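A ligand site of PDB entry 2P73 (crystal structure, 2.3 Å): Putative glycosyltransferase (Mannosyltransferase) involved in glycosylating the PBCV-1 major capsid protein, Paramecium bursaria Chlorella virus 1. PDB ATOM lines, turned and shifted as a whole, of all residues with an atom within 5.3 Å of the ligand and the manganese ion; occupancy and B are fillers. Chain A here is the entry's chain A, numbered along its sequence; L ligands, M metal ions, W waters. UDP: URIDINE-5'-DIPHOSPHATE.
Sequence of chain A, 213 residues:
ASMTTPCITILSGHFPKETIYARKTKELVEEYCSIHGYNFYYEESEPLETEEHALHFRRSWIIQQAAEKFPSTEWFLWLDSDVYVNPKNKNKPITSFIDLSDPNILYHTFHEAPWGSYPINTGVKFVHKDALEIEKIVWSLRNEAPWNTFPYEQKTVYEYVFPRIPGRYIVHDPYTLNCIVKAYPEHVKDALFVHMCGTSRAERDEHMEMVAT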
ATOM      1  N   GLY A  13     -22.933  -6.078  15.607  1.00  0.00           N
ATOM      2  CA  GLY A  13     -22.901  -7.399  16.198  1.00  0.00           C
ATOM      3  C   GLY A  13     -21.655  -7.540  17.026  1.00  0.00           C
ATOM      4  O   GLY A  13     -20.637  -6.893  16.754  1.00  0.00           O
ATOM      5  N   HIS A  14     -21.718  -8.378  18.046  1.00  0.00           N
ATOM      6  CA  HIS A  14     -20.592  -8.577  18.948  1.00  0.00           C
ATOM      7  C   HIS A  14     -20.636  -9.937  19.599  1.00  0.00           C
ATOM      8  O   HIS A  14     -21.671 -10.332  20.171  1.00  0.00           O
ATOM      9  CB  HIS A  14     -20.563  -7.482  20.023  1.00  0.00           C
ATOM     10  CG  HIS A  14     -19.345  -7.528  20.884  1.00  0.00           C
ATOM     11  ND1 HIS A  14     -18.164  -6.909  20.542  1.00  0.00           N
ATOM     12  CD2 HIS A  14     -19.126  -8.114  22.092  1.00  0.00           C
ATOM     13  CE1 HIS A  14     -17.265  -7.113  21.497  1.00  0.00           C
ATOM     14  NE2 HIS A  14     -17.820  -7.835  22.449  1.00  0.00           N
ATOM     15  N   PHE A  15     -19.522 -10.646  19.508  1.00  0.00           N
ATOM     16  CA  PHE A  15     -19.280 -11.854  20.279  1.00  0.00           C
ATOM     17  C   PHE A  15     -18.207 -11.574  21.316  1.00  0.00           C
ATOM     18  O   PHE A  15     -17.121 -11.091  20.968  1.00  0.00           O
ATOM     19  CB  PHE A  15     -18.851 -13.030  19.384  1.00  0.00           C
ATOM     20  CG  PHE A  15     -18.432 -14.248  20.157  1.00  0.00           C
ATOM     21  CD1 PHE A  15     -17.114 -14.404  20.583  1.00  0.00           C
ATOM     22  CD2 PHE A  15     -19.367 -15.231  20.501  1.00  0.00           C
ATOM     23  CE1 PHE A  15     -16.717 -15.526  21.333  1.00  0.00           C
ATOM     24  CE2 PHE A  15     -18.997 -16.365  21.236  1.00  0.00           C
ATOM     25  CZ  PHE A  15     -17.657 -16.512  21.655  1.00  0.00           C
ATOM     26  N   PRO A  16     -18.470 -11.897  22.594  1.00  0.00           N
ATOM     27  CA  PRO A  16     -19.701 -12.492  23.118  1.00  0.00           C
ATOM     28  C   PRO A  16     -20.829 -11.477  23.345  1.00  0.00           C
ATOM     29  O   PRO A  16     -20.568 -10.302  23.657  1.00  0.00           O
ATOM     30  CB  PRO A  16     -19.258 -13.098  24.447  1.00  0.00           C
ATOM     31  CG  PRO A  16     -18.166 -12.213  24.915  1.00  0.00           C
ATOM     32  CD  PRO A  16     -17.467 -11.691  23.667  1.00  0.00           C
ATOM     33  N   TYR A  21     -20.632  -3.174  27.292  1.00  0.00           N
ATOM     34  CA  TYR A  21     -20.555  -1.985  26.484  1.00  0.00           C
ATOM     35  C   TYR A  21     -21.189  -2.196  25.119  1.00  0.00           C
ATOM     36  O   TYR A  21     -21.696  -1.261  24.534  1.00  0.00           O
ATOM     37  CB  TYR A  21     -19.104  -1.479  26.337  1.00  0.00           C
ATOM     38  CG  TYR A  21     -18.247  -2.233  25.341  1.00  0.00           C
ATOM     39  CD1 TYR A  21     -18.282  -1.910  23.977  1.00  0.00           C
ATOM     40  CD2 TYR A  21     -17.394  -3.241  25.754  1.00  0.00           C
ATOM     41  CE1 TYR A  21     -17.506  -2.596  23.040  1.00  0.00           C
ATOM     42  CE2 TYR A  21     -16.593  -3.932  24.830  1.00  0.00           C
ATOM     43  CZ  TYR A  21     -16.660  -3.600  23.482  1.00  0.00           C
ATOM     44  OH  TYR A  21     -15.872  -4.281  22.588  1.00  0.00           O
ATOM     45  N   LEU A  55     -13.620 -12.893  13.834  1.00  0.00           N
ATOM     46  CA  LEU A  55     -14.577 -11.957  14.427  1.00  0.00           C
ATOM     47  C   LEU A  55     -14.495 -10.584  13.754  1.00  0.00           C
ATOM     48  O   LEU A  55     -15.519  -9.928  13.546  1.00  0.00           O
ATOM     49  CB  LEU A  55     -14.373 -11.837  15.940  1.00  0.00           C
ATOM     50  CG  LEU A  55     -14.523 -13.117  16.781  1.00  0.00           C
ATOM     51  CD1 LEU A  55     -14.053 -12.834  18.194  1.00  0.00           C
ATOM     52  CD2 LEU A  55     -15.953 -13.640  16.790  1.00  0.00           C
ATOM     53  N   HIS A  56     -13.283 -10.159  13.403  1.00  0.00           N
ATOM     54  CA  HIS A  56     -13.099  -8.907  12.700  1.00  0.00           C
ATOM     55  C   HIS A  56     -13.618  -8.925  11.269  1.00  0.00           C
ATOM     56  O   HIS A  56     -14.035  -7.899  10.772  1.00  0.00           O
ATOM     57  CB  HIS A  56     -11.634  -8.493  12.713  1.00  0.00           C
ATOM     58  CG  HIS A  56     -11.220  -7.822  13.980  1.00  0.00           C
ATOM     59  ND1 HIS A  56     -10.874  -6.489  14.053  1.00  0.00           N
ATOM     60  CD2 HIS A  56     -11.106  -8.307  15.245  1.00  0.00           C
ATOM     61  CE1 HIS A  56     -10.529  -6.192  15.292  1.00  0.00           C
ATOM     62  NE2 HIS A  56     -10.664  -7.275  16.042  1.00  0.00           N
ATOM     63  N   ARG A  59     -18.262  -8.813   9.986  1.00  0.00           N
ATOM     64  CA  ARG A  59     -19.093  -7.761   9.414  1.00  0.00           C
ATOM     65  C   ARG A  59     -19.429  -8.005   7.954  1.00  0.00           C
ATOM     66  O   ARG A  59     -20.441  -7.497   7.471  1.00  0.00           O
ATOM     67  CB  ARG A  59     -18.416  -6.411   9.582  1.00  0.00           C
ATOM     68  CG  ARG A  59     -17.310  -6.056   8.569  1.00  0.00           C
ATOM     69  CD  ARG A  59     -16.506  -4.872   9.114  1.00  0.00           C
ATOM     70  NE  ARG A  59     -15.742  -5.293  10.267  1.00  0.00           N
ATOM     71  CZ  ARG A  59     -15.050  -4.498  11.087  1.00  0.00           C
ATOM     72  NH1 ARG A  59     -15.034  -3.187  10.907  1.00  0.00           N
ATOM     73  NH2 ARG A  59     -14.379  -5.032  12.086  1.00  0.00           N
ATOM     74  N   TRP A  78     -22.195  -0.306   8.484  1.00  0.00           N
ATOM     75  CA  TRP A  78     -21.567  -1.045   9.545  1.00  0.00           C
ATOM     76  C   TRP A  78     -21.024  -0.090  10.594  1.00  0.00           C
ATOM     77  O   TRP A  78     -20.325   0.870  10.266  1.00  0.00           O
ATOM     78  CB  TRP A  78     -20.413  -1.926   9.026  1.00  0.00           C
ATOM     79  CG  TRP A  78     -19.681  -2.549  10.192  1.00  0.00           C
ATOM     80  CD1 TRP A  78     -18.494  -2.107  10.769  1.00  0.00           C
ATOM     81  CD2 TRP A  78     -20.087  -3.689  10.948  1.00  0.00           C
ATOM     82  NE1 TRP A  78     -18.150  -2.929  11.818  1.00  0.00           N
ATOM     83  CE2 TRP A  78     -19.112  -3.896  11.958  1.00  0.00           C
ATOM     84  CE3 TRP A  78     -21.179  -4.571  10.865  1.00  0.00           C
ATOM     85  CZ2 TRP A  78     -19.210  -4.953  12.882  1.00  0.00           C
ATOM     86  CZ3 TRP A  78     -21.255  -5.619  11.783  1.00  0.00           C
ATOM     87  CH2 TRP A  78     -20.277  -5.806  12.767  1.00  0.00           C
ATOM     88  N   LEU A  79     -21.409  -0.345  11.839  1.00  0.00           N
ATOM     89  CA  LEU A  79     -20.836   0.314  13.003  1.00  0.00           C
ATOM     90  C   LEU A  79     -20.296  -0.748  13.927  1.00  0.00           C
ATOM     91  O   LEU A  79     -20.987  -1.717  14.268  1.00  0.00           O
ATOM     92  CB  LEU A  79     -21.889   1.119  13.759  1.00  0.00           C
ATOM     93  CG  LEU A  79     -22.678   2.204  13.034  1.00  0.00           C
ATOM     94  CD1 LEU A  79     -23.707   2.784  13.964  1.00  0.00           C
ATOM     95  CD2 LEU A  79     -21.763   3.269  12.473  1.00  0.00           C
ATOM     96  N   ASP A  80     -19.035  -0.586  14.299  1.00  0.00           N
ATOM     97  CA  ASP A  80     -18.427  -1.449  15.282  1.00  0.00           C
ATOM     98  C   ASP A  80     -19.221  -1.380  16.580  1.00  0.00           C
ATOM     99  O   ASP A  80     -19.821  -0.338  16.908  1.00  0.00           O
ATOM    100  CB  ASP A  80     -17.006  -1.016  15.554  1.00  0.00           C
ATOM    101  CG  ASP A  80     -15.971  -1.706  14.655  1.00  0.00           C
ATOM    102  OD1 ASP A  80     -16.317  -2.537  13.801  1.00  0.00           O
ATOM    103  OD2 ASP A  80     -14.784  -1.417  14.808  1.00  0.00           O
ATOM    104  N   SER A  81     -19.194  -2.487  17.325  1.00  0.00           N
ATOM    105  CA  SER A  81     -19.778  -2.595  18.641  1.00  0.00           C
ATOM    106  C   SER A  81     -19.259  -1.605  19.688  1.00  0.00           C
ATOM    107  O   SER A  81     -19.880  -1.447  20.752  1.00  0.00           O
ATOM    108  CB  SER A  81     -19.617  -4.032  19.166  1.00  0.00           C
ATOM    109  OG  SER A  81     -18.249  -4.387  19.240  1.00  0.00           O
ATOM    110  N   ASP A  82     -18.138  -0.942  19.417  1.00  0.00           N
ATOM    111  CA  ASP A  82     -17.638   0.102  20.328  1.00  0.00           C
ATOM    112  C   ASP A  82     -17.835   1.499  19.742  1.00  0.00           C
ATOM    113  O   ASP A  82     -17.134   2.450  20.111  1.00  0.00           O
ATOM    114  CB  ASP A  82     -16.166  -0.143  20.669  1.00  0.00           C
ATOM    115  CG  ASP A  82     -15.299  -0.233  19.437  1.00  0.00           C
ATOM    116  OD1 ASP A  82     -15.833  -0.512  18.347  1.00  0.00           O
ATOM    117  OD2 ASP A  82     -14.076  -0.015  19.539  1.00  0.00           O
ATOM    118  N   VAL A  83     -18.762   1.591  18.788  1.00  0.00           N
ATOM    119  CA  VAL A  83     -19.195   2.861  18.249  1.00  0.00           C
ATOM    120  C   VAL A  83     -20.612   3.127  18.779  1.00  0.00           C
ATOM    121  O   VAL A  83     -21.503   2.264  18.666  1.00  0.00           O
ATOM    122  CB  VAL A  83     -19.248   2.854  16.690  1.00  0.00           C
ATOM    123  CG1 VAL A  83     -19.845   4.159  16.165  1.00  0.00           C
ATOM    124  CG2 VAL A  83     -17.853   2.651  16.061  1.00  0.00           C
ATOM    125  N   GLY A 123     -14.368   0.817  11.090  1.00  0.00           N
ATOM    126  CA  GLY A 123     -15.318   0.728  12.209  1.00  0.00           C
ATOM    127  C   GLY A 123     -16.651   1.414  11.932  1.00  0.00           C
ATOM    128  O   GLY A 123     -17.639   1.127  12.573  1.00  0.00           O
ATOM    129  N   HIS A 195     -16.191   6.574  18.237  1.00  0.00           N
ATOM    130  CA  HIS A 195     -15.544   5.242  18.195  1.00  0.00           C
ATOM    131  C   HIS A 195     -14.552   5.116  19.350  1.00  0.00           C
ATOM    132  O   HIS A 195     -13.587   5.876  19.413  1.00  0.00           O
ATOM    133  CB  HIS A 195     -14.772   5.055  16.883  1.00  0.00           C
ATOM    134  CG  HIS A 195     -14.357   3.641  16.594  1.00  0.00           C
ATOM    135  ND1 HIS A 195     -13.838   3.278  15.365  1.00  0.00           N
ATOM    136  CD2 HIS A 195     -14.400   2.495  17.328  1.00  0.00           C
ATOM    137  CE1 HIS A 195     -13.582   1.979  15.363  1.00  0.00           C
ATOM    138  NE2 HIS A 195     -13.915   1.475  16.535  1.00  0.00           N
ATOM    139  N   MET A 196     -14.800   4.157  20.231  1.00  0.00           N
ATOM    140  CA  MET A 196     -13.885   3.890  21.342  1.00  0.00           C
ATOM    141  C   MET A 196     -12.806   2.926  20.908  1.00  0.00           C
ATOM    142  O   MET A 196     -12.524   1.939  21.584  1.00  0.00           O
ATOM    143  CB  MET A 196     -14.630   3.290  22.518  1.00  0.00           C
ATOM    144  CG  MET A 196     -15.724   4.165  23.092  1.00  0.00           C
ATOM    145  SD  MET A 196     -16.570   3.290  24.408  1.00  0.00           S
ATOM    146  CE  MET A 196     -17.440   2.005  23.512  1.00  0.00           C
ATOM    147  N   CYS A 197     -12.204   3.212  19.762  1.00  0.00           N
ATOM    148  CA  CYS A 197     -11.239   2.338  19.077  1.00  0.00           C
ATOM    149  C   CYS A 197      -9.929   2.084  19.854  1.00  0.00           C
ATOM    150  O   CYS A 197      -9.331   3.021  20.409  1.00  0.00           O
ATOM    151  CB  CYS A 197     -10.923   2.949  17.726  1.00  0.00           C
ATOM    152  SG  CYS A 197      -9.635   2.099  16.831  1.00  0.00           S
ATOM    153  N   GLY A 198      -9.487   0.828  19.847  1.00  0.00           N
ATOM    154  CA  GLY A 198      -8.181   0.456  20.425  1.00  0.00           C
ATOM    155  C   GLY A 198      -8.044   0.594  21.934  1.00  0.00           C
ATOM    156  O   GLY A 198      -6.976   0.971  22.442  1.00  0.00           O
ATOM    157  N   THR A 199      -9.143   0.302  22.641  1.00  0.00           N
ATOM    158  CA  THR A 199      -9.200   0.298  24.108  1.00  0.00           C
ATOM    159  C   THR A 199      -9.779  -1.041  24.560  1.00  0.00           C
ATOM    160  O   THR A 199     -10.396  -1.751  23.762  1.00  0.00           O
ATOM    161  CB  THR A 199     -10.095   1.429  24.658  1.00  0.00           C
ATOM    162  OG1 THR A 199     -11.316   1.455  23.917  1.00  0.00           O
ATOM    163  CG2 THR A 199      -9.402   2.791  24.542  1.00  0.00           C
ATOM    164  N   ARG A 204     -13.798   0.328  27.849  1.00  0.00           N
ATOM    165  CA  ARG A 204     -15.026   0.617  27.103  1.00  0.00           C
ATOM    166  C   ARG A 204     -16.276   0.533  27.986  1.00  0.00           C
ATOM    167  O   ARG A 204     -17.186   1.358  27.874  1.00  0.00           O
ATOM    168  CB  ARG A 204     -15.159  -0.306  25.885  1.00  0.00           C
ATOM    169  CG  ARG A 204     -14.120  -0.049  24.798  1.00  0.00           C
ATOM    170  CD  ARG A 204     -14.104  -1.129  23.737  1.00  0.00           C
ATOM    171  NE  ARG A 204     -13.146  -0.840  22.663  1.00  0.00           N
ATOM    172  CZ  ARG A 204     -12.733  -1.736  21.773  1.00  0.00           C
ATOM    173  NH1 ARG A 204     -13.195  -2.972  21.807  1.00  0.00           N
ATOM    174  NH2 ARG A 204     -11.831  -1.385  20.864  1.00  0.00           N
HETATM  175  N1  UDP L   1     -15.309  -8.234  17.609  1.00  0.00           N
HETATM  176  C2  UDP L   1     -16.029  -9.136  18.385  1.00  0.00           C
HETATM  177  N3  UDP L   1     -15.510  -9.591  19.568  1.00  0.00           N
HETATM  178  C4  UDP L   1     -14.294  -9.116  20.013  1.00  0.00           C
HETATM  179  C5  UDP L   1     -13.576  -8.202  19.231  1.00  0.00           C
HETATM  180  C6  UDP L   1     -13.991  -7.992  17.911  1.00  0.00           C
HETATM  181  O2  UDP L   1     -17.101  -9.596  18.046  1.00  0.00           O
HETATM  182  O4  UDP L   1     -13.879  -9.547  21.093  1.00  0.00           O
HETATM  183  C1' UDP L   1     -15.905  -7.771  16.329  1.00  0.00           C
HETATM  184  C2' UDP L   1     -17.013  -6.810  16.693  1.00  0.00           C
HETATM  185  O2' UDP L   1     -18.127  -7.088  15.856  1.00  0.00           O
HETATM  186  C3' UDP L   1     -16.415  -5.438  16.437  1.00  0.00           C
HETATM  187  C4' UDP L   1     -15.299  -5.692  15.416  1.00  0.00           C
HETATM  188  O4' UDP L   1     -14.976  -7.080  15.510  1.00  0.00           O
HETATM  189  O3' UDP L   1     -17.413  -4.550  15.964  1.00  0.00           O
HETATM  190  C5' UDP L   1     -14.031  -4.885  15.658  1.00  0.00           C
HETATM  191  O5' UDP L   1     -13.608  -5.074  16.987  1.00  0.00           O
HETATM  192  PA  UDP L   1     -12.974  -3.854  17.803  1.00  0.00           P
HETATM  193  O1A UDP L   1     -13.877  -2.679  17.760  1.00  0.00           O
HETATM  194  O2A UDP L   1     -12.602  -4.198  19.172  1.00  0.00           O
HETATM  195  O3A UDP L   1     -11.673  -3.439  16.929  1.00  0.00           O
HETATM  196  PB  UDP L   1     -10.899  -2.033  17.079  1.00  0.00           P
HETATM  197  O1B UDP L   1     -11.691  -0.859  16.614  1.00  0.00           O
HETATM  198  O2B UDP L   1     -10.595  -1.775  18.514  1.00  0.00           O
HETATM  199  O3B UDP L   1      -9.653  -2.074  16.252  1.00  0.00           O
HETATM  200 MN    MN M   1     -14.009  -0.591  16.927  1.00  0.00          MN
HETATM  201  O   HOH W   1     -16.633  -7.665  12.603  1.00  0.00           O
HETATM  202  O   HOH W   2     -15.990  -3.671  19.978  1.00  0.00           O
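Water W2 lies within hydrogen-bond range of OG of Ser 81 (2.5 Å), OH of Tyr 21 (2.7 Å) and NH1 of Arg 204 (3.4 Å).
NE of Arg 59 lies within hydrogen-bond range of O of His 56 (3.2 Å). The side-chain hydroxyl of Tyr 21 is in hydrogen-bond range of the guanidinium group of Arg 204, at 3.1 Å. The backbone NH (N) of Asp 80 sits at hydrogen-bond distance from the backbone carbonyl oxygen (O) of Gly 123 (2.8 Å). NE of Arg 204 sits at hydrogen-bond distance from O of Met 196 (3.0 Å). A ring nitrogen (ND1) of His 14 is in hydrogen-bond range of the side-chain hydroxyl (OG) of Ser 81 (2.8 Å). OD2 of Asp 82 lies close to NH2 of Arg 204 (2.9 Å). The indole nitrogen of Trp 78 lies within hydrogen-bond range of the side-chain carboxylate of Asp 80, at 2.7 Å. The backbone carbonyl oxygen (O) of Asp 82 lies within hydrogen-bond range of the backbone NH (N) of Met 196.
The manganese ion is bound by NE2 of His 195 (2.1 Å), O1A of the ligand (2.3 Å), OD1 of Asp 82 (2.3 Å), O1B of the ligand (2.4 Å), OD2 of Asp 80 (2.4 Å) and OD2 of Asp 82 (2.7 Å). The manganese ion has six donor atoms within binding distance.
His 14 touches the ligand. O of Leu 55 touches O4' of the ligand (3.5 Å). His 56 touches the ligand. Arg 59 touches the ligand. Trp 78 touches the ligand (CZ2 to O3', 3.6 Å). Within 4 Å of the ligand: Gly 13, His 14, Phe 15, Leu 55, His 56, Arg 59, Trp 78, Asp 80, Ser 81, Asp 82, His 195, Cys 197, Gly 198 and Arg 204.
An oxygen (O2B) of the ligand is in hydrogen-bond range of the backbone NH (N) of Gly 198 (3.1 Å). An oxygen (O2) of the ligand is in hydrogen-bond range of the backbone NH of Phe 15 (3.0 Å). OG of Ser 81 sits at hydrogen-bond distance from O3' of the ligand, 3.4 Å away. A nitrogen (N3) of the ligand lies within hydrogen-bond range of the backbone carbonyl oxygen of Phe 15 (2.6 Å). The backbone NH of Ser 81 lies within hydrogen-bond range of an oxygen (O3') of the ligand (3.0 Å). An oxygen (O1B) of the ligand lies close to the side-chain sulfur (SG) of Cys 197 (3.6 Å). The guanidinium group of Arg 204 is in salt-bridge range of an oxygen (O2B) of the ligand (2.7 Å). The backbone carbonyl oxygen (O) of Gly 13 sits at hydrogen-bond distance from an oxygen (O2') of the ligand, 2.7 Å away.
Three residues have an atom within 4 Å of the manganese ion: Asp 80, Asp 82 and His 195. The nearest printed residue that does not touch the manganese ion is Arg 204 (4.6 Å).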
